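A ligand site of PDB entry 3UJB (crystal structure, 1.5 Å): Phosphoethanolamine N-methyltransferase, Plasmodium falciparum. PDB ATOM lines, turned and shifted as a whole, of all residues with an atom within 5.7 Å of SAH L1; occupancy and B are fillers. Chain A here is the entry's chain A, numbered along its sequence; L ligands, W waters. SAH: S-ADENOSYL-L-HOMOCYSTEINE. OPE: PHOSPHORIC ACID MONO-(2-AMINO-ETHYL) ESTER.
The backbone carbonyl oxygen of Asp 85 is in hydrogen-bond range of the backbone NH of Asn 109, 3.0 Å away.
N of Gly 65 lies within hydrogen-bond range of OD2 of Asp 85, at 2.9 Å.
N of Gly 63 lies within hydrogen-bond range of O of Ile 84 (2.8 Å).
N of Leu 112 is in hydrogen-bond range of OD1 of Asp 110 (3.0 Å).
N of Ile 86 lies close to O of Asn 109, at 3.4 Å.
NE2 of His 132 is in hydrogen-bond range of OH of Tyr 19.
O of Leu 14 sits at hydrogen-bond distance from N of Tyr 19 (2.9 Å).
N of Ser 64 lies within hydrogen-bond range of O of Ile 84 (3.0 Å).
The side-chain hydroxyl (OG) of Ser 37 lies within hydrogen-bond range of an oxygen (O) of SAH L1 (2.5 Å).
OD1 of Asp 85 is in hydrogen-bond range of O2' of SAH L1 (2.6 Å).
N of SAH L1 is in hydrogen-bond range of O of Gly 63, 2.8 Å away.
OXT of SAH L1 lies within hydrogen-bond range of N of Ile 36, 2.9 Å away.
The side-chain carboxylate (OD1) of Asp 110 lies within hydrogen-bond range of a nitrogen (N6) of SAH L1, 2.9 Å away.
A nitrogen (N) of SAH L1 sits at hydrogen-bond distance from the backbone carbonyl oxygen of Arg 127 (3.0 Å).
The backbone NH (N) of Ile 111 sits at hydrogen-bond distance from a nitrogen (N1) of SAH L1 (3.1 Å).
The backbone NH (N) of Ile 86 sits at hydrogen-bond distance from a nitrogen (N3) of SAH L1 (3.2 Å).
The side-chain sulfur of Cys 87 lies within hydrogen-bond range of an oxygen (O2') of SAH L1.
OH of Tyr 19 sits close to SD of SAH L1.
OH of Tyr 19 lies within hydrogen-bond range of N of OPE L2, 2.5 Å away.
Leu 14 touches SAH L1.
Tyr 35 touches SAH L1.
Ser 64 touches SAH L1.
CA of Gly 65 touches CB of SAH L1 (3.7 Å).
Ile 90 touches SAH L1.
Asn 109 touches SAH L1.
Asp 128 touches SAH L1 (O to C5', 3.5 Å).
Ala 129 touches SAH L1 (CB to O4', 3.4 Å).
CD2 of His 132 touches C8 of SAH L1 (3.6 Å).
Leu 133 touches SAH L1.
Hydrophobic or aromatic side chains within 4 Å of SAH L1: Leu 14, Tyr 19, Ile 36, Ile 86, Ile 90, Ile 111, Ala 129, His 132 and Leu 133.
The nearest printed residue that does not touch SAH L1 is Ile 84 (4.2 Å).
Water W5 lies within hydrogen-bond range of OXT of SAH L1 (2.7 Å), N of Leu 66 (2.8 Å), O of Asn 34 (2.9 Å) and O of Ser 64 (3.5 Å).
Water W4 lies within hydrogen-bond range of O of SAH L1 (2.8 Å), OG of Ser 37 (3.2 Å) and NH1 of Arg 127 (3.3 Å).
Water W2 bridges OD2 of Asp 61 and N of SAH L1.
Water W6 lies within hydrogen-bond range of the backbone carbonyl oxygen of Ser 64 (3.2 Å) and an oxygen (OXT) of SAH L1 (3.5 Å).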
ATOM      1  N   LEU A  14      10.025 -15.173 -32.897  1.00  0.00           N
ATOM      2  CA  LEU A  14      10.066 -15.136 -31.444  1.00  0.00           C
ATOM      3  C   LEU A  14      10.583 -13.791 -30.902  1.00  0.00           C
ATOM      4  O   LEU A  14      10.015 -13.224 -29.979  1.00  0.00           O
ATOM      5  CB  LEU A  14      10.910 -16.293 -30.906  1.00  0.00           C
ATOM      6  CG  LEU A  14      10.349 -17.703 -31.146  1.00  0.00           C
ATOM      7  CD1 LEU A  14      11.400 -18.715 -30.701  1.00  0.00           C
ATOM      8  CD2 LEU A  14       9.050 -17.925 -30.397  1.00  0.00           C
ATOM      9  N   TYR A  19       8.838 -12.878 -27.403  1.00  0.00           N
ATOM     10  CA  TYR A  19      10.012 -12.569 -26.605  1.00  0.00           C
ATOM     11  C   TYR A  19      10.751 -11.301 -27.039  1.00  0.00           C
ATOM     12  O   TYR A  19      11.980 -11.282 -27.117  1.00  0.00           O
ATOM     13  CB  TYR A  19      10.964 -13.764 -26.551  1.00  0.00           C
ATOM     14  CG  TYR A  19      10.320 -15.058 -26.080  1.00  0.00           C
ATOM     15  CD1 TYR A  19       9.864 -15.195 -24.769  1.00  0.00           C
ATOM     16  CD2 TYR A  19      10.197 -16.134 -26.931  1.00  0.00           C
ATOM     17  CE1 TYR A  19       9.284 -16.377 -24.331  1.00  0.00           C
ATOM     18  CE2 TYR A  19       9.616 -17.326 -26.502  1.00  0.00           C
ATOM     19  CZ  TYR A  19       9.166 -17.438 -25.207  1.00  0.00           C
ATOM     20  OH  TYR A  19       8.598 -18.637 -24.804  1.00  0.00           O
ATOM     21  N   ASN A  34      15.061 -13.866 -13.313  1.00  0.00           N
ATOM     22  CA  ASN A  34      15.871 -14.800 -14.066  1.00  0.00           C
ATOM     23  C   ASN A  34      15.095 -15.949 -14.738  1.00  0.00           C
ATOM     24  O   ASN A  34      15.694 -16.785 -15.305  1.00  0.00           O
ATOM     25  CB  ASN A  34      17.029 -15.368 -13.266  1.00  0.00           C
ATOM     26  CG  ASN A  34      17.902 -14.311 -12.702  1.00  0.00           C
ATOM     27  OD1 ASN A  34      18.147 -13.336 -13.313  1.00  0.00           O
ATOM     28  ND2 ASN A  34      18.342 -14.514 -11.511  1.00  0.00           N
ATOM     29  N   TYR A  35      13.788 -15.887 -14.645  1.00  0.00           N
ATOM     30  CA  TYR A  35      12.929 -16.929 -15.206  1.00  0.00           C
ATOM     31  C   TYR A  35      11.871 -16.368 -16.148  1.00  0.00           C
ATOM     32  O   TYR A  35      11.340 -15.288 -15.923  1.00  0.00           O
ATOM     33  CB  TYR A  35      12.237 -17.701 -14.088  1.00  0.00           C
ATOM     34  CG  TYR A  35      13.184 -18.578 -13.315  1.00  0.00           C
ATOM     35  CD1 TYR A  35      13.792 -18.122 -12.142  1.00  0.00           C
ATOM     36  CD2 TYR A  35      13.504 -19.856 -13.765  1.00  0.00           C
ATOM     37  CE1 TYR A  35      14.685 -18.934 -11.442  1.00  0.00           C
ATOM     38  CE2 TYR A  35      14.384 -20.669 -13.072  1.00  0.00           C
ATOM     39  CZ  TYR A  35      14.969 -20.202 -11.916  1.00  0.00           C
ATOM     40  OH  TYR A  35      15.856 -21.007 -11.222  1.00  0.00           O
ATOM     41  N   ILE A  36      11.574 -17.133 -17.199  1.00  0.00           N
ATOM     42  CA  ILE A  36      10.439 -16.821 -18.052  1.00  0.00           C
ATOM     43  C   ILE A  36       9.594 -18.064 -18.310  1.00  0.00           C
ATOM     44  O   ILE A  36       9.000 -18.225 -19.385  1.00  0.00           O
ATOM     45  CB  ILE A  36      10.830 -16.117 -19.365  1.00  0.00           C
ATOM     46  CG1 ILE A  36      11.890 -16.922 -20.122  1.00  0.00           C
ATOM     47  CG2 ILE A  36      11.362 -14.706 -19.070  1.00  0.00           C
ATOM     48  CD1 ILE A  36      12.435 -16.174 -21.338  1.00  0.00           C
ATOM     49  N   SER A  37       9.545 -18.944 -17.311  1.00  0.00           N
ATOM     50  CA  SER A  37       8.642 -20.077 -17.386  1.00  0.00           C
ATOM     51  C   SER A  37       8.074 -20.466 -16.028  1.00  0.00           C
ATOM     52  O   SER A  37       8.574 -20.035 -14.978  1.00  0.00           O
ATOM     53  CB  SER A  37       9.329 -21.284 -18.007  1.00  0.00           C
ATOM     54  OG  SER A  37      10.149 -21.921 -17.045  1.00  0.00           O
ATOM     55  N   ASP A  61      21.311 -26.951 -21.066  1.00  0.00           N
ATOM     56  CA  ASP A  61      19.967 -26.402 -20.852  1.00  0.00           C
ATOM     57  C   ASP A  61      19.442 -25.922 -22.207  1.00  0.00           C
ATOM     58  O   ASP A  61      19.948 -24.949 -22.767  1.00  0.00           O
ATOM     59  CB  ASP A  61      20.016 -25.219 -19.862  1.00  0.00           C
ATOM     60  CG  ASP A  61      18.631 -24.654 -19.545  1.00  0.00           C
ATOM     61  OD1 ASP A  61      17.675 -24.971 -20.268  1.00  0.00           O
ATOM     62  OD2 ASP A  61      18.498 -23.865 -18.564  1.00  0.00           O
ATOM     63  N   ILE A  62      18.452 -26.629 -22.751  1.00  0.00           N
ATOM     64  CA  ILE A  62      17.883 -26.300 -24.050  1.00  0.00           C
ATOM     65  C   ILE A  62      16.760 -25.279 -23.911  1.00  0.00           C
ATOM     66  O   ILE A  62      15.711 -25.569 -23.335  1.00  0.00           O
ATOM     67  CB  ILE A  62      17.319 -27.560 -24.726  1.00  0.00           C
ATOM     68  CG1 ILE A  62      18.451 -28.538 -25.037  1.00  0.00           C
ATOM     69  CG2 ILE A  62      16.558 -27.198 -26.000  1.00  0.00           C
ATOM     70  CD1 ILE A  62      17.965 -29.891 -25.548  1.00  0.00           C
ATOM     71  N   GLY A  63      16.975 -24.072 -24.454  1.00  0.00           N
ATOM     72  CA  GLY A  63      16.039 -22.970 -24.270  1.00  0.00           C
ATOM     73  C   GLY A  63      16.295 -22.282 -22.936  1.00  0.00           C
ATOM     74  O   GLY A  63      15.381 -22.113 -22.136  1.00  0.00           O
ATOM     75  N   SER A  64      17.543 -21.875 -22.728  1.00  0.00           N
ATOM     76  CA  SER A  64      17.992 -21.429 -21.405  1.00  0.00           C
ATOM     77  C   SER A  64      17.453 -20.080 -20.931  1.00  0.00           C
ATOM     78  O   SER A  64      17.578 -19.747 -19.754  1.00  0.00           O
ATOM     79  CB  SER A  64      19.524 -21.426 -21.357  1.00  0.00           C
ATOM     80  OG  SER A  64      20.060 -20.756 -22.484  1.00  0.00           O
ATOM     81  N   GLY A  65      16.853 -19.304 -21.812  1.00  0.00           N
ATOM     82  CA  GLY A  65      16.187 -18.094 -21.369  1.00  0.00           C
ATOM     83  C   GLY A  65      17.102 -17.084 -20.696  1.00  0.00           C
ATOM     84  O   GLY A  65      18.187 -16.819 -21.186  1.00  0.00           O
ATOM     85  N   LEU A  66      16.640 -16.532 -19.579  1.00  0.00           N
ATOM     86  CA  LEU A  66      17.421 -15.522 -18.851  1.00  0.00           C
ATOM     87  C   LEU A  66      18.488 -16.146 -17.979  1.00  0.00           C
ATOM     88  O   LEU A  66      19.248 -15.434 -17.305  1.00  0.00           O
ATOM     89  CB  LEU A  66      16.512 -14.626 -18.013  1.00  0.00           C
ATOM     90  CG  LEU A  66      15.561 -13.715 -18.798  1.00  0.00           C
ATOM     91  CD1 LEU A  66      14.593 -13.021 -17.851  1.00  0.00           C
ATOM     92  CD2 LEU A  66      16.372 -12.708 -19.600  1.00  0.00           C
ATOM     93  N   ILE A  84      21.632 -22.978 -24.241  1.00  0.00           N
ATOM     94  CA  ILE A  84      21.439 -22.574 -25.637  1.00  0.00           C
ATOM     95  C   ILE A  84      20.060 -21.948 -25.761  1.00  0.00           C
ATOM     96  O   ILE A  84      19.085 -22.495 -25.256  1.00  0.00           O
ATOM     97  CB  ILE A  84      21.492 -23.775 -26.589  1.00  0.00           C
ATOM     98  CG1 ILE A  84      22.841 -24.489 -26.503  1.00  0.00           C
ATOM     99  CG2 ILE A  84      21.235 -23.318 -28.024  1.00  0.00           C
ATOM    100  CD1 ILE A  84      23.954 -23.738 -27.204  1.00  0.00           C
ATOM    101  N   ASP A  85      20.006 -20.799 -26.424  1.00  0.00           N
ATOM    102  CA  ASP A  85      18.726 -20.155 -26.675  1.00  0.00           C
ATOM    103  C   ASP A  85      18.775 -19.460 -28.022  1.00  0.00           C
ATOM    104  O   ASP A  85      19.780 -18.837 -28.367  1.00  0.00           O
ATOM    105  CB  ASP A  85      18.397 -19.159 -25.568  1.00  0.00           C
ATOM    106  CG  ASP A  85      16.921 -18.836 -25.527  1.00  0.00           C
ATOM    107  OD1 ASP A  85      16.441 -18.125 -26.428  1.00  0.00           O
ATOM    108  OD2 ASP A  85      16.247 -19.322 -24.601  1.00  0.00           O
ATOM    109  N   ILE A  86      17.678 -19.562 -28.768  1.00  0.00           N
ATOM    110  CA  ILE A  86      17.638 -19.056 -30.132  1.00  0.00           C
ATOM    111  C   ILE A  86      17.502 -17.521 -30.198  1.00  0.00           C
ATOM    112  O   ILE A  86      17.847 -16.910 -31.202  1.00  0.00           O
ATOM    113  CB  ILE A  86      16.510 -19.745 -30.947  1.00  0.00           C
ATOM    114  CG1 ILE A  86      16.717 -19.574 -32.441  1.00  0.00           C
ATOM    115  CG2 ILE A  86      15.137 -19.242 -30.523  1.00  0.00           C
ATOM    116  CD1 ILE A  86      15.750 -20.376 -33.287  1.00  0.00           C
ATOM    117  N   CYS A  87      16.986 -16.921 -29.137  1.00  0.00           N
ATOM    118  CA  CYS A  87      16.763 -15.475 -29.119  1.00  0.00           C
ATOM    119  C   CYS A  87      18.002 -14.724 -28.627  1.00  0.00           C
ATOM    120  O   CYS A  87      18.353 -14.800 -27.453  1.00  0.00           O
ATOM    121  CB  CYS A  87      15.553 -15.121 -28.242  1.00  0.00           C
ATOM    122  SG  CYS A  87      13.965 -15.624 -28.989  1.00  0.00           S
ATOM    123  N   ILE A  90      17.618 -12.335 -25.657  1.00  0.00           N
ATOM    124  CA  ILE A  90      17.495 -13.004 -24.370  1.00  0.00           C
ATOM    125  C   ILE A  90      18.851 -13.499 -23.860  1.00  0.00           C
ATOM    126  O   ILE A  90      19.193 -13.348 -22.687  1.00  0.00           O
ATOM    127  CB  ILE A  90      16.531 -14.199 -24.472  1.00  0.00           C
ATOM    128  CG1 ILE A  90      15.101 -13.716 -24.736  1.00  0.00           C
ATOM    129  CG2 ILE A  90      16.584 -15.037 -23.204  1.00  0.00           C
ATOM    130  CD1 ILE A  90      14.102 -14.856 -24.886  1.00  0.00           C
ATOM    131  N   ASN A 109      21.817 -19.711 -30.344  1.00  0.00           N
ATOM    132  CA  ASN A 109      21.789 -20.638 -31.469  1.00  0.00           C
ATOM    133  C   ASN A 109      20.477 -21.448 -31.441  1.00  0.00           C
ATOM    134  O   ASN A 109      19.865 -21.547 -30.476  1.00  0.00           O
ATOM    135  CB  ASN A 109      23.009 -21.568 -31.486  1.00  0.00           C
ATOM    136  CG  ASN A 109      24.104 -21.120 -32.486  1.00  0.00           C
ATOM    137  OD1 ASN A 109      23.821 -20.462 -33.463  1.00  0.00           O
ATOM    138  ND2 ASN A 109      25.322 -21.382 -32.157  1.00  0.00           N
ATOM    139  N   ASP A 110      20.117 -21.957 -32.590  1.00  0.00           N
ATOM    140  CA  ASP A 110      18.957 -22.828 -32.732  1.00  0.00           C
ATOM    141  C   ASP A 110      19.425 -24.209 -32.301  1.00  0.00           C
ATOM    142  O   ASP A 110      20.414 -24.709 -32.833  1.00  0.00           O
ATOM    143  CB  ASP A 110      18.537 -22.845 -34.201  1.00  0.00           C
ATOM    144  CG  ASP A 110      17.316 -23.712 -34.483  1.00  0.00           C
ATOM    145  OD1 ASP A 110      16.795 -24.403 -33.577  1.00  0.00           O
ATOM    146  OD2 ASP A 110      16.882 -23.711 -35.658  1.00  0.00           O
ATOM    147  N   ILE A 111      18.757 -24.821 -31.324  1.00  0.00           N
ATOM    148  CA  ILE A 111      19.204 -26.132 -30.879  1.00  0.00           C
ATOM    149  C   ILE A 111      19.160 -27.167 -32.005  1.00  0.00           C
ATOM    150  O   ILE A 111      19.919 -28.135 -31.995  1.00  0.00           O
ATOM    151  CB  ILE A 111      18.404 -26.625 -29.643  1.00  0.00           C
ATOM    152  CG1 ILE A 111      19.070 -27.859 -29.016  1.00  0.00           C
ATOM    153  CG2 ILE A 111      16.936 -26.910 -29.997  1.00  0.00           C
ATOM    154  CD1 ILE A 111      20.433 -27.560 -28.405  1.00  0.00           C
ATOM    155  N   LEU A 112      18.279 -26.952 -32.972  1.00  0.00           N
ATOM    156  CA  LEU A 112      18.094 -27.923 -34.053  1.00  0.00           C
ATOM    157  C   LEU A 112      19.285 -28.011 -35.007  1.00  0.00           C
ATOM    158  O   LEU A 112      19.445 -29.005 -35.724  1.00  0.00           O
ATOM    159  CB  LEU A 112      16.821 -27.612 -34.829  1.00  0.00           C
ATOM    160  CG  LEU A 112      15.551 -27.861 -34.009  1.00  0.00           C
ATOM    161  CD1 LEU A 112      14.334 -27.308 -34.742  1.00  0.00           C
ATOM    162  CD2 LEU A 112      15.379 -29.345 -33.704  1.00  0.00           C
ATOM    163  N   SER A 126      15.466 -29.166 -19.992  1.00  0.00           N
ATOM    164  CA  SER A 126      14.715 -28.179 -20.771  1.00  0.00           C
ATOM    165  C   SER A 126      13.423 -27.878 -20.065  1.00  0.00           C
ATOM    166  O   SER A 126      12.721 -28.793 -19.643  1.00  0.00           O
ATOM    167  CB  SER A 126      14.448 -28.703 -22.183  1.00  0.00           C
ATOM    168  OG  SER A 126      13.858 -27.691 -22.997  1.00  0.00           O
ATOM    169  N   ARG A 127      13.122 -26.590 -19.938  1.00  0.00           N
ATOM    170  CA  ARG A 127      11.938 -26.141 -19.228  1.00  0.00           C
ATOM    171  C   ARG A 127      11.074 -25.247 -20.113  1.00  0.00           C
ATOM    172  O   ARG A 127      11.426 -24.095 -20.409  1.00  0.00           O
ATOM    173  CB  ARG A 127      12.339 -25.396 -17.948  1.00  0.00           C
ATOM    174  CG  ARG A 127      13.233 -26.218 -17.008  1.00  0.00           C
ATOM    175  CD  ARG A 127      12.446 -27.327 -16.281  1.00  0.00           C
ATOM    176  NE  ARG A 127      11.249 -26.747 -15.688  1.00  0.00           N
ATOM    177  CZ  ARG A 127      11.253 -26.031 -14.561  1.00  0.00           C
ATOM    178  NH1 ARG A 127      12.372 -25.871 -13.867  1.00  0.00           N
ATOM    179  NH2 ARG A 127      10.118 -25.487 -14.123  1.00  0.00           N
ATOM    180  N   ASP A 128       9.942 -25.797 -20.534  1.00  0.00           N
ATOM    181  CA  ASP A 128       8.929 -25.064 -21.313  1.00  0.00           C
ATOM    182  C   ASP A 128       9.533 -24.370 -22.527  1.00  0.00           C
ATOM    183  O   ASP A 128       9.277 -23.180 -22.772  1.00  0.00           O
ATOM    184  CB  ASP A 128       8.156 -24.065 -20.442  1.00  0.00           C
ATOM    185  CG  ASP A 128       7.446 -24.724 -19.260  1.00  0.00           C
ATOM    186  OD1 ASP A 128       7.404 -25.976 -19.187  1.00  0.00           O
ATOM    187  OD2 ASP A 128       6.909 -23.976 -18.420  1.00  0.00           O
ATOM    188  N   ALA A 129      10.291 -25.126 -23.313  1.00  0.00           N
ATOM    189  CA  ALA A 129      10.903 -24.602 -24.533  1.00  0.00           C
ATOM    190  C   ALA A 129      10.552 -25.415 -25.777  1.00  0.00           C
ATOM    191  O   ALA A 129      10.477 -24.891 -26.882  1.00  0.00           O
ATOM    192  CB  ALA A 129      12.411 -24.542 -24.385  1.00  0.00           C
ATOM    193  N   LEU A 131       7.852 -26.813 -26.691  1.00  0.00           N
ATOM    194  CA  LEU A 131       6.539 -26.465 -27.275  1.00  0.00           C
ATOM    195  C   LEU A 131       6.661 -25.582 -28.530  1.00  0.00           C
ATOM    196  O   LEU A 131       5.745 -25.532 -29.350  1.00  0.00           O
ATOM    197  CB  LEU A 131       5.653 -25.739 -26.245  1.00  0.00           C
ATOM    198  CG  LEU A 131       6.028 -24.319 -25.839  1.00  0.00           C
ATOM    199  CD1 LEU A 131       4.969 -23.770 -24.912  1.00  0.00           C
ATOM    200  CD2 LEU A 131       7.397 -24.287 -25.158  1.00  0.00           C
ATOM    201  N   HIS A 132       7.778 -24.874 -28.660  1.00  0.00           N
ATOM    202  CA  HIS A 132       8.026 -24.044 -29.830  1.00  0.00           C
ATOM    203  C   HIS A 132       8.339 -24.856 -31.083  1.00  0.00           C
ATOM    204  O   HIS A 132       8.242 -24.351 -32.207  1.00  0.00           O
ATOM    205  CB  HIS A 132       9.151 -23.036 -29.536  1.00  0.00           C
ATOM    206  CG  HIS A 132       8.758 -21.971 -28.543  1.00  0.00           C
ATOM    207  ND1 HIS A 132       7.806 -21.017 -28.821  1.00  0.00           N
ATOM    208  CD2 HIS A 132       9.198 -21.720 -27.297  1.00  0.00           C
ATOM    209  CE1 HIS A 132       7.675 -20.217 -27.771  1.00  0.00           C
ATOM    210  NE2 HIS A 132       8.507 -20.627 -26.833  1.00  0.00           N
ATOM    211  N   LEU A 133       8.698 -26.127 -30.899  1.00  0.00           N
ATOM    212  CA  LEU A 133       9.091 -26.970 -32.028  1.00  0.00           C
ATOM    213  C   LEU A 133       7.935 -27.741 -32.657  1.00  0.00           C
ATOM    214  O   LEU A 133       7.064 -28.246 -31.965  1.00  0.00           O
ATOM    215  CB  LEU A 133      10.173 -27.969 -31.581  1.00  0.00           C
ATOM    216  CG  LEU A 133      11.604 -27.458 -31.490  1.00  0.00           C
ATOM    217  CD1 LEU A 133      11.722 -26.202 -30.624  1.00  0.00           C
ATOM    218  CD2 LEU A 133      12.551 -28.554 -30.972  1.00  0.00           C
HETATM  219  N   SAH L   1      13.885 -22.403 -19.835  1.00  0.00           N
HETATM  220  CA  SAH L   1      13.799 -20.941 -19.580  1.00  0.00           C
HETATM  221  CB  SAH L   1      13.146 -20.208 -20.808  1.00  0.00           C
HETATM  222  CG  SAH L   1      11.676 -20.600 -21.038  1.00  0.00           C
HETATM  223  SD  SAH L   1      10.904 -19.710 -22.426  1.00  0.00           S
HETATM  224  C   SAH L   1      13.091 -20.716 -18.315  1.00  0.00           C
HETATM  225  O   SAH L   1      12.535 -21.642 -17.761  1.00  0.00           O
HETATM  226  OXT SAH L   1      12.988 -19.593 -17.875  1.00  0.00           O
HETATM  227  C5' SAH L   1      11.375 -20.630 -23.914  1.00  0.00           C
HETATM  228  C4' SAH L   1      12.670 -20.404 -24.477  1.00  0.00           C
HETATM  229  O4' SAH L   1      12.855 -21.358 -25.546  1.00  0.00           O
HETATM  230  C3' SAH L   1      12.762 -19.055 -25.094  1.00  0.00           C
HETATM  231  O3' SAH L   1      13.769 -18.290 -24.440  1.00  0.00           O
HETATM  232  C2' SAH L   1      13.053 -19.318 -26.521  1.00  0.00           C
HETATM  233  O2' SAH L   1      13.919 -18.374 -27.131  1.00  0.00           O
HETATM  234  C1' SAH L   1      13.630 -20.696 -26.503  1.00  0.00           C
HETATM  235  N9  SAH L   1      13.588 -21.417 -27.827  1.00  0.00           N
HETATM  236  C8  SAH L   1      12.526 -21.580 -28.630  1.00  0.00           C
HETATM  237  N7  SAH L   1      12.915 -22.283 -29.695  1.00  0.00           N
HETATM  238  C5  SAH L   1      14.213 -22.588 -29.569  1.00  0.00           C
HETATM  239  C6  SAH L   1      15.131 -23.280 -30.379  1.00  0.00           C
HETATM  240  N6  SAH L   1      14.750 -23.843 -31.572  1.00  0.00           N
HETATM  241  N1  SAH L   1      16.403 -23.394 -29.945  1.00  0.00           N
HETATM  242  C2  SAH L   1      16.796 -22.849 -28.788  1.00  0.00           C
HETATM  243  N3  SAH L   1      15.939 -22.170 -27.987  1.00  0.00           N
HETATM  244  C4  SAH L   1      14.660 -22.019 -28.365  1.00  0.00           C
HETATM  245  CA  OPE L   2       5.111 -18.593 -21.274  1.00  0.00           C
HETATM  246  CB  OPE L   2       6.536 -18.315 -21.604  1.00  0.00           C
HETATM  247  O1  OPE L   2       2.271 -17.026 -22.074  1.00  0.00           O
HETATM  248  O2  OPE L   2       2.392 -19.177 -20.855  1.00  0.00           O
HETATM  249  O3  OPE L   2       2.127 -19.198 -23.347  1.00  0.00           O
HETATM  250  O4  OPE L   2       4.253 -18.515 -22.341  1.00  0.00           O
HETATM  251  N   OPE L   2       6.981 -18.808 -22.865  1.00  0.00           N
HETATM  252  P   OPE L   2       2.703 -18.485 -22.150  1.00  0.00           P
HETATM  253  O   HOH W   1      11.811 -22.730 -32.257  1.00  0.00           O
HETATM  254  O   HOH W   2      15.842 -23.185 -17.914  1.00  0.00           O
HETATM  255  O   HOH W   3      15.120 -24.741 -20.705  1.00  0.00           O
HETATM  256  O   HOH W   4      12.572 -22.918 -15.274  1.00  0.00           O
HETATM  257  O   HOH W   5      15.202 -18.094 -17.794  1.00  0.00           O
HETATM  258  O   HOH W   6      16.219 -20.530 -16.949  1.00  0.00           O
